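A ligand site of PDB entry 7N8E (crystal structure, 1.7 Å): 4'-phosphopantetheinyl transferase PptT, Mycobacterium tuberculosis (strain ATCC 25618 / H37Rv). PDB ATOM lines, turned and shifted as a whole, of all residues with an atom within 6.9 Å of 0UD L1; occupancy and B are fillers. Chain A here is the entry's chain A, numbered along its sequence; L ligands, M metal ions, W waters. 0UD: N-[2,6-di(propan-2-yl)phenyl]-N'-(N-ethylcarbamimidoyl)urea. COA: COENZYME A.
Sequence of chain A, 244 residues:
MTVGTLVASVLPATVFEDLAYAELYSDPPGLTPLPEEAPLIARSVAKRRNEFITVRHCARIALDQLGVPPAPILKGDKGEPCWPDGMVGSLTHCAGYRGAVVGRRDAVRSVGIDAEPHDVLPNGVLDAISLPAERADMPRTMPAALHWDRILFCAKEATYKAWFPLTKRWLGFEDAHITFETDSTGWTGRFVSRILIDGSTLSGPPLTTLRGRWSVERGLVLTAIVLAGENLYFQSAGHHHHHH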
ATOM      1  N   LYS A  78      32.320   4.851   8.337  1.00  0.00           N
ATOM      2  CA  LYS A  78      32.433   3.412   8.495  1.00  0.00           C
ATOM      3  C   LYS A  78      31.380   2.642   7.689  1.00  0.00           C
ATOM      4  O   LYS A  78      31.236   1.433   7.870  1.00  0.00           O
ATOM      5  CB  LYS A  78      32.343   3.022   9.969  1.00  0.00           C
ATOM      6  CG  LYS A  78      33.614   3.279  10.757  1.00  0.00           C
ATOM      7  CD  LYS A  78      34.749   2.407  10.245  1.00  0.00           C
ATOM      8  N   ASP A 114      19.074  -7.629  11.379  1.00  0.00           N
ATOM      9  CA  ASP A 114      19.919  -8.428  10.498  1.00  0.00           C
ATOM     10  C   ASP A 114      19.087  -9.578   9.932  1.00  0.00           C
ATOM     11  O   ASP A 114      18.184 -10.091  10.583  1.00  0.00           O
ATOM     12  CB  ASP A 114      21.137  -9.013  11.226  1.00  0.00           C
ATOM     13  CG  ASP A 114      22.164  -9.566  10.269  1.00  0.00           C
ATOM     14  OD1 ASP A 114      22.646  -8.814   9.405  1.00  0.00           O
ATOM     15  OD2 ASP A 114      22.520 -10.757  10.400  1.00  0.00           O
ATOM     16  N   ILE A 129      32.922 -16.220  15.983  1.00  0.00           N
ATOM     17  CA  ILE A 129      31.864 -15.265  16.286  1.00  0.00           C
ATOM     18  C   ILE A 129      31.158 -15.541  17.606  1.00  0.00           C
ATOM     19  O   ILE A 129      30.270 -14.777  17.994  1.00  0.00           O
ATOM     20  CB  ILE A 129      30.822 -15.186  15.152  1.00  0.00           C
ATOM     21  CG1 ILE A 129      30.146 -16.546  14.928  1.00  0.00           C
ATOM     22  CG2 ILE A 129      31.501 -14.726  13.862  1.00  0.00           C
ATOM     23  CD1 ILE A 129      28.853 -16.734  15.687  1.00  0.00           C
ATOM     24  N   PHE A 153      24.905 -15.692  15.080  1.00  0.00           N
ATOM     25  CA  PHE A 153      25.595 -14.693  14.272  1.00  0.00           C
ATOM     26  C   PHE A 153      24.667 -13.538  13.931  1.00  0.00           C
ATOM     27  O   PHE A 153      25.078 -12.377  14.018  1.00  0.00           O
ATOM     28  CB  PHE A 153      26.126 -15.346  12.993  1.00  0.00           C
ATOM     29  CG  PHE A 153      26.752 -14.361  12.042  1.00  0.00           C
ATOM     30  CD1 PHE A 153      27.923 -13.711  12.385  1.00  0.00           C
ATOM     31  CD2 PHE A 153      26.182 -14.122  10.794  1.00  0.00           C
ATOM     32  CE1 PHE A 153      28.508 -12.803  11.516  1.00  0.00           C
ATOM     33  CE2 PHE A 153      26.763 -13.227   9.914  1.00  0.00           C
ATOM     34  CZ  PHE A 153      27.941 -12.561  10.290  1.00  0.00           C
ATOM     35  N   ALA A 155      22.120 -12.434  15.626  1.00  0.00           N
ATOM     36  CA  ALA A 155      21.902 -11.624  16.817  1.00  0.00           C
ATOM     37  C   ALA A 155      23.113 -10.766  17.126  1.00  0.00           C
ATOM     38  O   ALA A 155      22.959  -9.612  17.546  1.00  0.00           O
ATOM     39  CB  ALA A 155      21.547 -12.522  18.014  1.00  0.00           C
ATOM     40  N   LYS A 156      24.323 -11.290  16.901  1.00  0.00           N
ATOM     41  CA  LYS A 156      25.512 -10.448  17.037  1.00  0.00           C
ATOM     42  C   LYS A 156      25.464  -9.266  16.079  1.00  0.00           C
ATOM     43  O   LYS A 156      25.854  -8.154  16.442  1.00  0.00           O
ATOM     44  CB  LYS A 156      26.779 -11.283  16.782  1.00  0.00           C
ATOM     45  CG  LYS A 156      26.931 -12.512  17.699  1.00  0.00           C
ATOM     46  CD  LYS A 156      27.806 -12.235  18.890  1.00  0.00           C
ATOM     47  CE  LYS A 156      27.918 -13.480  19.774  1.00  0.00           C
ATOM     48  NZ  LYS A 156      28.954 -13.316  20.839  1.00  0.00           N
ATOM     49  N   GLU A 157      24.973  -9.484  14.854  1.00  0.00           N
ATOM     50  CA  GLU A 157      24.991  -8.411  13.866  1.00  0.00           C
ATOM     51  C   GLU A 157      23.966  -7.336  14.218  1.00  0.00           C
ATOM     52  O   GLU A 157      24.266  -6.135  14.114  1.00  0.00           O
ATOM     53  CB  GLU A 157      24.761  -8.969  12.465  1.00  0.00           C
ATOM     54  CG  GLU A 157      25.884  -9.881  12.003  1.00  0.00           C
ATOM     55  CD  GLU A 157      27.195  -9.145  11.989  1.00  0.00           C
ATOM     56  OE1 GLU A 157      27.474  -8.447  10.982  1.00  0.00           O
ATOM     57  OE2 GLU A 157      27.939  -9.223  12.983  1.00  0.00           O
ATOM     58  N   ALA A 158      22.753  -7.726  14.629  1.00  0.00           N
ATOM     59  CA  ALA A 158      21.788  -6.739  15.063  1.00  0.00           C
ATOM     60  C   ALA A 158      22.306  -5.949  16.263  1.00  0.00           C
ATOM     61  O   ALA A 158      22.096  -4.742  16.363  1.00  0.00           O
ATOM     62  CB  ALA A 158      20.448  -7.416  15.411  1.00  0.00           C
ATOM     63  N   THR A 159      23.023  -6.633  17.168  1.00  0.00           N
ATOM     64  CA  THR A 159      23.589  -5.958  18.333  1.00  0.00           C
ATOM     65  C   THR A 159      24.562  -4.864  17.909  1.00  0.00           C
ATOM     66  O   THR A 159      24.469  -3.729  18.369  1.00  0.00           O
ATOM     67  CB  THR A 159      24.279  -6.964  19.247  1.00  0.00           C
ATOM     68  OG1 THR A 159      23.325  -7.908  19.736  1.00  0.00           O
ATOM     69  CG2 THR A 159      24.912  -6.246  20.431  1.00  0.00           C
ATOM     70  N   TYR A 160      25.498  -5.197  17.015  1.00  0.00           N
ATOM     71  CA  TYR A 160      26.457  -4.194  16.557  1.00  0.00           C
ATOM     72  C   TYR A 160      25.767  -3.040  15.849  1.00  0.00           C
ATOM     73  O   TYR A 160      26.158  -1.878  16.003  1.00  0.00           O
ATOM     74  CB  TYR A 160      27.477  -4.842  15.621  1.00  0.00           C
ATOM     75  CG  TYR A 160      28.574  -3.886  15.227  1.00  0.00           C
ATOM     76  CD1 TYR A 160      29.302  -3.205  16.200  1.00  0.00           C
ATOM     77  CD2 TYR A 160      28.868  -3.641  13.890  1.00  0.00           C
ATOM     78  CE1 TYR A 160      30.300  -2.316  15.850  1.00  0.00           C
ATOM     79  CE2 TYR A 160      29.863  -2.742  13.540  1.00  0.00           C
ATOM     80  CZ  TYR A 160      30.578  -2.095  14.520  1.00  0.00           C
ATOM     81  OH  TYR A 160      31.567  -1.209  14.168  1.00  0.00           O
ATOM     82  N   LYS A 161      24.733  -3.343  15.049  1.00  0.00           N
ATOM     83  CA  LYS A 161      24.082  -2.288  14.281  1.00  0.00           C
ATOM     84  C   LYS A 161      23.282  -1.348  15.182  1.00  0.00           C
ATOM     85  O   LYS A 161      23.118  -0.164  14.848  1.00  0.00           O
ATOM     86  CB  LYS A 161      23.164  -2.910  13.219  1.00  0.00           C
ATOM     87  CG  LYS A 161      23.924  -3.475  12.027  1.00  0.00           C
ATOM     88  CD  LYS A 161      22.912  -3.965  10.987  1.00  0.00           C
ATOM     89  CE  LYS A 161      23.543  -4.825   9.940  1.00  0.00           C
ATOM     90  NZ  LYS A 161      22.427  -5.417   9.111  1.00  0.00           N
ATOM     91  N   TRP A 170      34.027   0.326  17.920  1.00  0.00           N
ATOM     92  CA  TRP A 170      34.041  -1.075  17.547  1.00  0.00           C
ATOM     93  C   TRP A 170      33.465  -1.933  18.667  1.00  0.00           C
ATOM     94  O   TRP A 170      33.640  -1.655  19.861  1.00  0.00           O
ATOM     95  CB  TRP A 170      35.475  -1.501  17.229  1.00  0.00           C
ATOM     96  CG  TRP A 170      35.637  -2.950  16.964  1.00  0.00           C
ATOM     97  CD1 TRP A 170      36.318  -3.860  17.727  1.00  0.00           C
ATOM     98  CD2 TRP A 170      35.084  -3.687  15.866  1.00  0.00           C
ATOM     99  NE1 TRP A 170      36.243  -5.110  17.147  1.00  0.00           N
ATOM    100  CE2 TRP A 170      35.476  -5.034  16.011  1.00  0.00           C
ATOM    101  CE3 TRP A 170      34.295  -3.341  14.760  1.00  0.00           C
ATOM    102  CZ2 TRP A 170      35.117  -6.028  15.102  1.00  0.00           C
ATOM    103  CZ3 TRP A 170      33.930  -4.325  13.859  1.00  0.00           C
ATOM    104  CH2 TRP A 170      34.348  -5.650  14.042  1.00  0.00           C
ATOM    105  N   LEU A 171      32.729  -2.971  18.284  1.00  0.00           N
ATOM    106  CA  LEU A 171      32.270  -4.005  19.202  1.00  0.00           C
ATOM    107  C   LEU A 171      32.655  -5.331  18.593  1.00  0.00           C
ATOM    108  O   LEU A 171      32.239  -5.641  17.475  1.00  0.00           O
ATOM    109  CB  LEU A 171      30.755  -3.918  19.430  1.00  0.00           C
ATOM    110  CG  LEU A 171      30.175  -4.916  20.427  1.00  0.00           C
ATOM    111  CD1 LEU A 171      30.549  -4.521  21.854  1.00  0.00           C
ATOM    112  CD2 LEU A 171      28.662  -5.018  20.263  1.00  0.00           C
ATOM    113  N   GLY A 172      33.512  -6.090  19.291  1.00  0.00           N
ATOM    114  CA  GLY A 172      33.939  -7.371  18.787  1.00  0.00           C
ATOM    115  C   GLY A 172      32.933  -8.470  19.066  1.00  0.00           C
ATOM    116  O   GLY A 172      32.049  -8.339  19.896  1.00  0.00           O
ATOM    117  N   PHE A 173      33.085  -9.585  18.341  1.00  0.00           N
ATOM    118  CA  PHE A 173      32.180 -10.712  18.567  1.00  0.00           C
ATOM    119  C   PHE A 173      32.338 -11.289  19.961  1.00  0.00           C
ATOM    120  O   PHE A 173      31.393 -11.847  20.507  1.00  0.00           O
ATOM    121  CB  PHE A 173      32.404 -11.780  17.498  1.00  0.00           C
ATOM    122  CG  PHE A 173      31.896 -11.386  16.161  1.00  0.00           C
ATOM    123  CD1 PHE A 173      30.556 -11.571  15.831  1.00  0.00           C
ATOM    124  CD2 PHE A 173      32.732 -10.797  15.238  1.00  0.00           C
ATOM    125  CE1 PHE A 173      30.074 -11.188  14.606  1.00  0.00           C
ATOM    126  CE2 PHE A 173      32.247 -10.395  14.001  1.00  0.00           C
ATOM    127  CZ  PHE A 173      30.908 -10.598  13.692  1.00  0.00           C
ATOM    128  N   GLU A 174      33.523 -11.132  20.559  1.00  0.00           N
ATOM    129  CA  GLU A 174      33.728 -11.592  21.923  1.00  0.00           C
ATOM    130  C   GLU A 174      33.258 -10.580  22.962  1.00  0.00           C
ATOM    131  O   GLU A 174      33.297 -10.888  24.159  1.00  0.00           O
ATOM    132  CB  GLU A 174      35.212 -11.934  22.130  1.00  0.00           C
ATOM    133  CG  GLU A 174      36.138 -10.726  22.305  1.00  0.00           C
ATOM    134  CD  GLU A 174      36.417  -9.954  21.025  1.00  0.00           C
ATOM    135  OE1 GLU A 174      37.123  -8.926  21.108  1.00  0.00           O
ATOM    136  OE2 GLU A 174      35.963 -10.376  19.940  1.00  0.00           O
ATOM    137  N   ASP A 175      32.815  -9.404  22.545  1.00  0.00           N
ATOM    138  CA  ASP A 175      32.446  -8.323  23.456  1.00  0.00           C
ATOM    139  C   ASP A 175      30.960  -8.308  23.819  1.00  0.00           C
ATOM    140  O   ASP A 175      30.529  -7.421  24.559  1.00  0.00           O
ATOM    141  CB  ASP A 175      32.832  -6.974  22.843  1.00  0.00           C
ATOM    142  CG  ASP A 175      34.330  -6.832  22.636  1.00  0.00           C
ATOM    143  OD1 ASP A 175      35.095  -7.465  23.398  1.00  0.00           O
ATOM    144  OD2 ASP A 175      34.742  -6.064  21.730  1.00  0.00           O
ATOM    145  N   ALA A 176      30.177  -9.259  23.305  1.00  0.00           N
ATOM    146  CA  ALA A 176      28.764  -9.340  23.640  1.00  0.00           C
ATOM    147  C   ALA A 176      28.402 -10.793  23.908  1.00  0.00           C
ATOM    148  O   ALA A 176      28.678 -11.662  23.079  1.00  0.00           O
ATOM    149  CB  ALA A 176      27.895  -8.768  22.515  1.00  0.00           C
ATOM    150  N   ILE A 178      25.297 -13.294  24.398  1.00  0.00           N
ATOM    151  CA  ILE A 178      23.894 -13.294  24.003  1.00  0.00           C
ATOM    152  C   ILE A 178      23.229 -14.571  24.512  1.00  0.00           C
ATOM    153  O   ILE A 178      23.722 -15.678  24.264  1.00  0.00           O
ATOM    154  CB  ILE A 178      23.733 -13.163  22.482  1.00  0.00           C
ATOM    155  CG1 ILE A 178      24.561 -11.976  21.961  1.00  0.00           C
ATOM    156  CG2 ILE A 178      22.258 -12.982  22.125  1.00  0.00           C
ATOM    157  CD1 ILE A 178      24.293 -11.661  20.488  1.00  0.00           C
HETATM  158  C01 0UD L   1      31.295 -10.164   9.511  1.00  0.00           C
HETATM  159  C02 0UD L   1      31.810  -8.751   9.894  1.00  0.00           C
HETATM  160  C03 0UD L   1      33.326  -8.719   9.789  1.00  0.00           C
HETATM  161  C04 0UD L   1      31.158  -7.612   9.145  1.00  0.00           C
HETATM  162  C05 0UD L   1      31.599  -7.327   7.861  1.00  0.00           C
HETATM  163  C06 0UD L   1      31.036  -6.305   7.130  1.00  0.00           C
HETATM  164  C07 0UD L   1      29.999  -5.549   7.663  1.00  0.00           C
HETATM  165  C08 0UD L   1      29.523  -5.792   8.945  1.00  0.00           C
HETATM  166  C09 0UD L   1      28.409  -4.887   9.421  1.00  0.00           C
HETATM  167  C10 0UD L   1      28.894  -3.753  10.302  1.00  0.00           C
HETATM  168  C11 0UD L   1      27.168  -5.508  10.005  1.00  0.00           C
HETATM  169  C12 0UD L   1      30.125  -6.852   9.699  1.00  0.00           C
HETATM  170  C14 0UD L   1      30.351  -6.859  12.176  1.00  0.00           C
HETATM  171  C16 0UD L   1      30.289  -7.089  14.655  1.00  0.00           C
HETATM  172  C18 0UD L   1      29.896  -7.537  17.094  1.00  0.00           C
HETATM  173  C19 0UD L   1      28.890  -8.275  17.980  1.00  0.00           C
HETATM  174  N13 0UD L   1      29.707  -7.222  11.002  1.00  0.00           N
HETATM  175  N15 0UD L   1      29.744  -7.383  13.363  1.00  0.00           N
HETATM  176  N17 0UD L   1      29.536  -7.703  15.697  1.00  0.00           N
HETATM  177  N20 0UD L   1      31.309  -6.358  14.900  1.00  0.00           N
HETATM  178  O21 0UD L   1      31.339  -6.145  12.171  1.00  0.00           O
HETATM  179  N1A COA L   2      26.605   0.424  12.049  1.00  0.00           N
HETATM  180  C2A COA L   2      25.288   0.270  11.642  1.00  0.00           C
HETATM  181  N3A COA L   2      24.798  -0.081  10.451  1.00  0.00           N
HETATM  182  C4A COA L   2      25.781  -0.320   9.516  1.00  0.00           C
HETATM  183  C5A COA L   2      27.185  -0.194   9.804  1.00  0.00           C
HETATM  184  C6A COA L   2      27.554   0.195  11.104  1.00  0.00           C
HETATM  185  N6A COA L   2      28.889   0.343  11.496  1.00  0.00           N
HETATM  186  N7A COA L   2      27.936  -0.496   8.645  1.00  0.00           N
HETATM  187  C8A COA L   2      26.979  -0.789   7.721  1.00  0.00           C
HETATM  188  N9A COA L   2      25.668  -0.686   8.207  1.00  0.00           N
HETATM  189  C1B COA L   2      24.370  -0.961   7.422  1.00  0.00           C
HETATM  190  C2B COA L   2      24.461  -0.355   5.997  1.00  0.00           C
HETATM  191  O2B COA L   2      23.325   0.372   5.770  1.00  0.00           O
HETATM  192  C3B COA L   2      24.682  -1.658   5.099  1.00  0.00           C
HETATM  193  O3B COA L   2      24.022  -1.634   3.954  1.00  0.00           O
HETATM  194  P3B COA L   2      24.460  -0.533   2.652  1.00  0.00           P
HETATM  195  O7A COA L   2      25.915  -0.835   2.536  1.00  0.00           O
HETATM  196  O8A COA L   2      23.586  -0.974   1.495  1.00  0.00           O
HETATM  197  O9A COA L   2      24.094   0.803   3.298  1.00  0.00           O
HETATM  198  C4B COA L   2      23.971  -2.677   5.964  1.00  0.00           C
HETATM  199  O4B COA L   2      24.202  -2.304   7.307  1.00  0.00           O
HETATM  200  C5B COA L   2      24.490  -4.040   5.614  1.00  0.00           C
HETATM  201  O5B COA L   2      23.805  -4.876   6.368  1.00  0.00           O
HETATM  202  P1A COA L   2      24.006  -6.544   6.108  1.00  0.00           P
HETATM  203  O1A COA L   2      25.523  -6.650   6.080  1.00  0.00           O
HETATM  204  O2A COA L   2      23.328  -7.152   7.297  1.00  0.00           O
HETATM  205  O3A COA L   2      23.361  -6.821   4.765  1.00  0.00           O
HETATM  206 MG    MG M   1      24.024  -8.900   8.020  1.00  0.00          MG
HETATM  207  O   HOH W   1      25.489  -7.855   9.162  1.00  0.00           O
HETATM  208  O   HOH W   2      32.978  -4.697  10.477  1.00  0.00           O
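O5B of COA L2 lies within hydrogen-bond range of NZ of Lys 161, at 3.1 Å. A nitrogen (N13) of 0UD L1 is in hydrogen-bond range of the side-chain carboxylate (OE1) of Glu 157, 2.5 Å away. A nitrogen (N20) of 0UD L1 sits at hydrogen-bond distance from the backbone carbonyl oxygen (O) of Leu 171 (2.8 Å).
The side-chain amino group (NZ) of Lys 156 is in hydrogen-bond range of the backbone carbonyl oxygen (O) of Ala 176 (2.8 Å). The backbone NH of Gly 172 sits at hydrogen-bond distance from the side-chain carboxylate of Asp 175 (2.7 Å). The side-chain amino group (NZ) of Lys 156 sits close to the backbone carbonyl oxygen (O) of Ile 129 (3.5 Å). The side-chain carboxylate (OD1) of Asp 114 sits close to the side-chain amino group (NZ) of Lys 161 (3.4 Å). The backbone carbonyl oxygen (O) of Phe 173 is in hydrogen-bond range of the side-chain amino group (NZ) of Lys 156 (2.9 Å).
Lys 156 touches 0UD L1 (O to C19, 3.4 Å). Tyr 160 touches 0UD L1 (CB to N17, 3.5 Å). Lys 161 touches 0UD L1. Trp 170 touches 0UD L1 (CH2 to N20, 3.2 Å). O of Gly 172 touches C18 of 0UD L1, 3.6 Å away. Phe 173 touches 0UD L1 (CZ to N15, 3.4 Å). Of the 19 residues printed, 8 come within 4 Å of 0UD L1.
Water W1 bridges OE1 of Glu 157 (2.8 Å) and O1A of COA L2 (3.3 Å).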
